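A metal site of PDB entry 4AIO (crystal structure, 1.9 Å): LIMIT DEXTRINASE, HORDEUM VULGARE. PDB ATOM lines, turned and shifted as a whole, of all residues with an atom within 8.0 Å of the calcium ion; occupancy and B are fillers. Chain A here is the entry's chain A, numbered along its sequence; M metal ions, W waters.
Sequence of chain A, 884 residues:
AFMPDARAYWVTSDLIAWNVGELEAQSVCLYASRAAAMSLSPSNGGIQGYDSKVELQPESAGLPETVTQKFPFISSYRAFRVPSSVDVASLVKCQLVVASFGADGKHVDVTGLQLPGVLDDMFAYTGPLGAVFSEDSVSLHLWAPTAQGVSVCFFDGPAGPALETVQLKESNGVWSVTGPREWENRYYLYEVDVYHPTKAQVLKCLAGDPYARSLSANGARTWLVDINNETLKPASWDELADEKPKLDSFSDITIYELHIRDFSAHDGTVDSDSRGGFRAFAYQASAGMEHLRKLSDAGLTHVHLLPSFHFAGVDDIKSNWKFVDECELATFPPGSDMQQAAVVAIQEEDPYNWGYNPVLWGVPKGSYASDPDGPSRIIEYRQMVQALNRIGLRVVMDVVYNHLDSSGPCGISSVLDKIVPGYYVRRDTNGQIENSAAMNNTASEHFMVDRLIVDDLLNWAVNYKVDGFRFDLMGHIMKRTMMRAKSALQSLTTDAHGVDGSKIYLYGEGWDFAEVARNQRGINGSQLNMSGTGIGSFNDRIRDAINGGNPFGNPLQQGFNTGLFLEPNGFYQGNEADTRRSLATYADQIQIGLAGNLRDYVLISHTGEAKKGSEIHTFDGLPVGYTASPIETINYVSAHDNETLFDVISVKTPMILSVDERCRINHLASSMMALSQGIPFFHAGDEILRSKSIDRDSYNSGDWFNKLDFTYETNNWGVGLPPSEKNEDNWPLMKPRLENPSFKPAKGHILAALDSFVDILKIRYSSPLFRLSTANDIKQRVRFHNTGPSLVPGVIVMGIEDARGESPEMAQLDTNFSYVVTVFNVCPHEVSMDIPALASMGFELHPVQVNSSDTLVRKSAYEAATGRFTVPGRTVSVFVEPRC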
ATOM      1  N   PRO A 245      31.150 -24.204  -7.128  1.00  0.00           N
ATOM      2  CA  PRO A 245      31.340 -25.388  -6.296  1.00  0.00           C
ATOM      3  C   PRO A 245      30.843 -26.629  -7.011  1.00  0.00           C
ATOM      4  O   PRO A 245      29.792 -26.591  -7.675  1.00  0.00           O
ATOM      5  CB  PRO A 245      30.464 -25.103  -5.068  1.00  0.00           C
ATOM      6  CG  PRO A 245      30.366 -23.618  -5.017  1.00  0.00           C
ATOM      7  CD  PRO A 245      30.322 -23.180  -6.451  1.00  0.00           C
ATOM      8  N   LYS A 246      31.586 -27.730  -6.888  1.00  0.00           N
ATOM      9  CA  LYS A 246      31.176 -28.987  -7.500  1.00  0.00           C
ATOM     10  C   LYS A 246      29.857 -29.454  -6.902  1.00  0.00           C
ATOM     11  O   LYS A 246      29.594 -29.256  -5.717  1.00  0.00           O
ATOM     12  CB  LYS A 246      32.251 -30.074  -7.345  1.00  0.00           C
ATOM     13  CG  LYS A 246      32.397 -30.634  -5.943  1.00  0.00           C
ATOM     14  N   THR A 254      22.081 -29.395   0.417  1.00  0.00           N
ATOM     15  CA  THR A 254      21.467 -28.867   1.636  1.00  0.00           C
ATOM     16  C   THR A 254      21.160 -27.391   1.397  1.00  0.00           C
ATOM     17  O   THR A 254      21.936 -26.688   0.738  1.00  0.00           O
ATOM     18  CB  THR A 254      22.380 -28.978   2.881  1.00  0.00           C
ATOM     19  OG1 THR A 254      23.730 -28.663   2.512  1.00  0.00           O
ATOM     20  CG2 THR A 254      22.325 -30.376   3.442  1.00  0.00           C
ATOM     21  N   LEU A 292      28.484 -17.780   7.199  1.00  0.00           N
ATOM     22  CA  LEU A 292      28.173 -18.602   6.016  1.00  0.00           C
ATOM     23  C   LEU A 292      29.347 -19.479   5.590  1.00  0.00           C
ATOM     24  O   LEU A 292      29.157 -20.634   5.186  1.00  0.00           O
ATOM     25  CB  LEU A 292      27.714 -17.735   4.832  1.00  0.00           C
ATOM     26  CG  LEU A 292      26.411 -16.947   4.996  1.00  0.00           C
ATOM     27  CD1 LEU A 292      26.023 -16.245   3.702  1.00  0.00           C
ATOM     28  CD2 LEU A 292      25.301 -17.886   5.434  1.00  0.00           C
ATOM     29  N   ARG A 293      30.557 -18.934   5.673  1.00  0.00           N
ATOM     30  CA  ARG A 293      31.754 -19.716   5.376  1.00  0.00           C
ATOM     31  C   ARG A 293      31.854 -20.924   6.282  1.00  0.00           C
ATOM     32  O   ARG A 293      32.228 -21.994   5.830  1.00  0.00           O
ATOM     33  CB  ARG A 293      33.033 -18.870   5.501  1.00  0.00           C
ATOM     34  CG  ARG A 293      33.310 -17.987   4.303  1.00  0.00           C
ATOM     35  N   LYS A 294      31.516 -20.745   7.557  1.00  0.00           N
ATOM     36  CA  LYS A 294      31.554 -21.833   8.533  1.00  0.00           C
ATOM     37  C   LYS A 294      30.571 -22.948   8.142  1.00  0.00           C
ATOM     38  O   LYS A 294      30.936 -24.127   8.120  1.00  0.00           O
ATOM     39  CB  LYS A 294      31.242 -21.318   9.944  1.00  0.00           C
ATOM     40  CG  LYS A 294      31.413 -22.374  11.026  1.00  0.00           C
ATOM     41  CD  LYS A 294      31.053 -21.822  12.397  1.00  0.00           C
ATOM     42  N   LEU A 295      29.331 -22.567   7.810  1.00  0.00           N
ATOM     43  CA  LEU A 295      28.312 -23.553   7.413  1.00  0.00           C
ATOM     44  C   LEU A 295      28.704 -24.221   6.083  1.00  0.00           C
ATOM     45  O   LEU A 295      28.613 -25.441   5.956  1.00  0.00           O
ATOM     46  CB  LEU A 295      26.939 -22.890   7.322  1.00  0.00           C
ATOM     47  CG  LEU A 295      26.509 -22.221   8.651  1.00  0.00           C
ATOM     48  CD1 LEU A 295      25.142 -21.554   8.520  1.00  0.00           C
ATOM     49  CD2 LEU A 295      26.503 -23.201   9.820  1.00  0.00           C
ATOM     50  N   SER A 296      29.158 -23.410   5.133  1.00  0.00           N
ATOM     51  CA  SER A 296      29.600 -23.902   3.838  1.00  0.00           C
ATOM     52  C   SER A 296      30.763 -24.903   3.938  1.00  0.00           C
ATOM     53  O   SER A 296      30.753 -25.942   3.265  1.00  0.00           O
ATOM     54  CB  SER A 296      30.028 -22.749   2.934  1.00  0.00           C
ATOM     55  OG  SER A 296      30.415 -23.251   1.670  1.00  0.00           O
ATOM     56  N   ASP A 297      31.749 -24.584   4.781  1.00  0.00           N
ATOM     57  CA  ASP A 297      32.871 -25.497   5.050  1.00  0.00           C
ATOM     58  C   ASP A 297      32.424 -26.806   5.692  1.00  0.00           C
ATOM     59  O   ASP A 297      32.955 -27.866   5.372  1.00  0.00           O
ATOM     60  CB  ASP A 297      33.928 -24.833   5.941  1.00  0.00           C
ATOM     61  CG  ASP A 297      34.712 -23.754   5.217  1.00  0.00           C
ATOM     62  OD1 ASP A 297      34.455 -23.488   4.010  1.00  0.00           O
ATOM     63  OD2 ASP A 297      35.600 -23.156   5.869  1.00  0.00           O
ATOM     64  N   ALA A 298      31.451 -26.739   6.589  1.00  0.00           N
ATOM     65  CA  ALA A 298      30.883 -27.933   7.209  1.00  0.00           C
ATOM     66  C   ALA A 298      30.116 -28.802   6.214  1.00  0.00           C
ATOM     67  O   ALA A 298      29.868 -29.978   6.479  1.00  0.00           O
ATOM     68  CB  ALA A 298      29.986 -27.536   8.387  1.00  0.00           C
ATOM     69  N   GLY A 299      29.724 -28.224   5.071  1.00  0.00           N
ATOM     70  CA  GLY A 299      29.044 -29.006   4.020  1.00  0.00           C
ATOM     71  C   GLY A 299      27.840 -28.369   3.347  1.00  0.00           C
ATOM     72  O   GLY A 299      27.344 -28.892   2.358  1.00  0.00           O
ATOM     73  N   LEU A 300      27.336 -27.244   3.883  1.00  0.00           N
ATOM     74  CA  LEU A 300      26.187 -26.549   3.277  1.00  0.00           C
ATOM     75  C   LEU A 300      26.464 -26.254   1.810  1.00  0.00           C
ATOM     76  O   LEU A 300      27.548 -25.743   1.474  1.00  0.00           O
ATOM     77  CB  LEU A 300      25.832 -25.262   4.046  1.00  0.00           C
ATOM     78  CG  LEU A 300      24.689 -24.428   3.435  1.00  0.00           C
ATOM     79  CD1 LEU A 300      23.349 -25.141   3.551  1.00  0.00           C
ATOM     80  CD2 LEU A 300      24.604 -23.016   4.021  1.00  0.00           C
ATOM     81  N   THR A 301      25.521 -26.571   0.927  1.00  0.00           N
ATOM     82  CA  THR A 301      25.770 -26.395  -0.500  1.00  0.00           C
ATOM     83  C   THR A 301      25.005 -25.241  -1.148  1.00  0.00           C
ATOM     84  O   THR A 301      25.496 -24.682  -2.110  1.00  0.00           O
ATOM     85  CB  THR A 301      25.473 -27.690  -1.306  1.00  0.00           C
ATOM     86  OG1 THR A 301      24.066 -27.983  -1.261  1.00  0.00           O
ATOM     87  CG2 THR A 301      26.275 -28.876  -0.761  1.00  0.00           C
ATOM     88  N   HIS A 302      23.826 -24.903  -0.632  1.00  0.00           N
ATOM     89  CA  HIS A 302      22.977 -23.890  -1.289  1.00  0.00           C
ATOM     90  C   HIS A 302      22.413 -22.878  -0.304  1.00  0.00           C
ATOM     91  O   HIS A 302      21.983 -23.233   0.788  1.00  0.00           O
ATOM     92  CB  HIS A 302      21.817 -24.562  -2.027  1.00  0.00           C
ATOM     93  CG  HIS A 302      22.229 -25.321  -3.282  1.00  0.00           C
ATOM     94  ND1 HIS A 302      22.991 -26.440  -3.256  1.00  0.00           N
ATOM     95  CD2 HIS A 302      21.902 -25.095  -4.629  1.00  0.00           C
ATOM     96  CE1 HIS A 302      23.176 -26.886  -4.528  1.00  0.00           C
ATOM     97  NE2 HIS A 302      22.492 -26.063  -5.368  1.00  0.00           N
ATOM     98  N   LEU A 388      29.188 -15.567  -3.165  1.00  0.00           N
ATOM     99  CA  LEU A 388      28.635 -16.781  -2.565  1.00  0.00           C
ATOM    100  C   LEU A 388      29.261 -18.066  -3.139  1.00  0.00           C
ATOM    101  O   LEU A 388      29.732 -18.930  -2.371  1.00  0.00           O
ATOM    102  CB  LEU A 388      27.108 -16.782  -2.628  1.00  0.00           C
ATOM    103  CG  LEU A 388      26.491 -15.821  -1.606  1.00  0.00           C
ATOM    104  CD1 LEU A 388      25.020 -15.558  -1.918  1.00  0.00           C
ATOM    105  CD2 LEU A 388      26.673 -16.345  -0.185  1.00  0.00           C
ATOM    106  N   ASN A 389      29.273 -18.174  -4.463  1.00  0.00           N
ATOM    107  CA  ASN A 389      29.974 -19.277  -5.170  1.00  0.00           C
ATOM    108  C   ASN A 389      31.409 -19.456  -4.681  1.00  0.00           C
ATOM    109  O   ASN A 389      31.870 -20.588  -4.489  1.00  0.00           O
ATOM    110  CB  ASN A 389      30.003 -19.048  -6.684  1.00  0.00           C
ATOM    111  CG  ASN A 389      28.652 -19.277  -7.376  1.00  0.00           C
ATOM    112  OD1 ASN A 389      28.502 -18.934  -8.541  1.00  0.00           O
ATOM    113  ND2 ASN A 389      27.692 -19.902  -6.675  1.00  0.00           N
ATOM    114  N   ILE A 391      32.745 -18.824  -1.723  1.00  0.00           N
ATOM    115  CA  ILE A 391      32.847 -19.482  -0.414  1.00  0.00           C
ATOM    116  C   ILE A 391      32.173 -20.861  -0.372  1.00  0.00           C
ATOM    117  O   ILE A 391      31.943 -21.416   0.702  1.00  0.00           O
ATOM    118  CB  ILE A 391      32.395 -18.565   0.748  1.00  0.00           C
ATOM    119  CG1 ILE A 391      30.910 -18.176   0.632  1.00  0.00           C
ATOM    120  CG2 ILE A 391      33.284 -17.329   0.833  1.00  0.00           C
ATOM    121  CD1 ILE A 391      30.272 -17.811   1.958  1.00  0.00           C
ATOM    122  N   GLY A 392      31.883 -21.427  -1.542  1.00  0.00           N
ATOM    123  CA  GLY A 392      31.369 -22.786  -1.647  1.00  0.00           C
ATOM    124  C   GLY A 392      29.853 -22.943  -1.596  1.00  0.00           C
ATOM    125  O   GLY A 392      29.335 -24.044  -1.325  1.00  0.00           O
ATOM    126  N   LEU A 393      29.148 -21.851  -1.877  1.00  0.00           N
ATOM    127  CA  LEU A 393      27.694 -21.869  -1.842  1.00  0.00           C
ATOM    128  C   LEU A 393      27.062 -21.533  -3.194  1.00  0.00           C
ATOM    129  O   LEU A 393      27.351 -20.497  -3.792  1.00  0.00           O
ATOM    130  CB  LEU A 393      27.167 -20.913  -0.753  1.00  0.00           C
ATOM    131  CG  LEU A 393      27.499 -21.291   0.699  1.00  0.00           C
ATOM    132  CD1 LEU A 393      27.227 -20.149   1.655  1.00  0.00           C
ATOM    133  CD2 LEU A 393      26.725 -22.537   1.098  1.00  0.00           C
ATOM    134  N   ARG A 394      26.176 -22.414  -3.656  1.00  0.00           N
ATOM    135  CA  ARG A 394      25.372 -22.167  -4.834  1.00  0.00           C
ATOM    136  C   ARG A 394      24.127 -21.345  -4.450  1.00  0.00           C
ATOM    137  O   ARG A 394      23.704 -21.383  -3.294  1.00  0.00           O
ATOM    138  CB  ARG A 394      25.016 -23.492  -5.526  1.00  0.00           C
ATOM    139  CG  ARG A 394      26.168 -24.033  -6.386  1.00  0.00           C
ATOM    140  CD  ARG A 394      25.811 -25.368  -7.005  1.00  0.00           C
ATOM    141  NE  ARG A 394      26.922 -25.922  -7.807  1.00  0.00           N
ATOM    142  CZ  ARG A 394      26.991 -25.875  -9.136  1.00  0.00           C
ATOM    143  NH1 ARG A 394      26.045 -25.280  -9.857  1.00  0.00           N
ATOM    144  NH2 ARG A 394      28.045 -26.408  -9.749  1.00  0.00           N
ATOM    145  N   TYR A 765      27.917 -35.073   5.583  1.00  0.00           N
ATOM    146  CA  TYR A 765      28.869 -35.092   4.490  1.00  0.00           C
ATOM    147  C   TYR A 765      30.066 -36.018   4.716  1.00  0.00           C
ATOM    148  O   TYR A 765      30.945 -36.127   3.861  1.00  0.00           O
ATOM    149  CB  TYR A 765      29.258 -33.651   4.126  1.00  0.00           C
ATOM    150  CG  TYR A 765      28.074 -32.955   3.466  1.00  0.00           C
ATOM    151  CD1 TYR A 765      27.819 -33.130   2.107  1.00  0.00           C
ATOM    152  CD2 TYR A 765      27.188 -32.166   4.214  1.00  0.00           C
ATOM    153  CE1 TYR A 765      26.736 -32.513   1.498  1.00  0.00           C
ATOM    154  CE2 TYR A 765      26.091 -31.550   3.601  1.00  0.00           C
ATOM    155  CZ  TYR A 765      25.876 -31.735   2.238  1.00  0.00           C
ATOM    156  OH  TYR A 765      24.811 -31.145   1.605  1.00  0.00           O
HETATM  157 CA    CA M   1      29.783 -25.436   0.855  1.00  0.00          CA
HETATM  158  O   HOH W   1      32.003 -25.948   0.128  1.00  0.00           O
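The side-chain hydroxyl (OG) of Ser 296 lies close to the backbone carbonyl oxygen (O) of Ile 391 (2.6 Å). The backbone NH of Leu 300 is in hydrogen-bond range of the backbone carbonyl oxygen of Leu 295.
Within 4 Å of the calcium ion: Ser 296, Leu 300 and Gly 392. The nearest printed residue that does not touch the calcium ion is Leu 393 (4.2 Å).
The calcium ion is bound by the backbone carbonyl oxygen (O) of Leu 300 (2.3 Å). Water W1 binds the calcium ion (2.4 Å). OG of Ser 296 binds the calcium ion, at 2.4 Å. The calcium ion is bound by the backbone carbonyl oxygen (O) of Gly 392 (2.6 Å). The backbone carbonyl oxygen (O) of Ser 296 binds the calcium ion, at 2.6 Å. The calcium ion has five donor atoms within binding distance.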
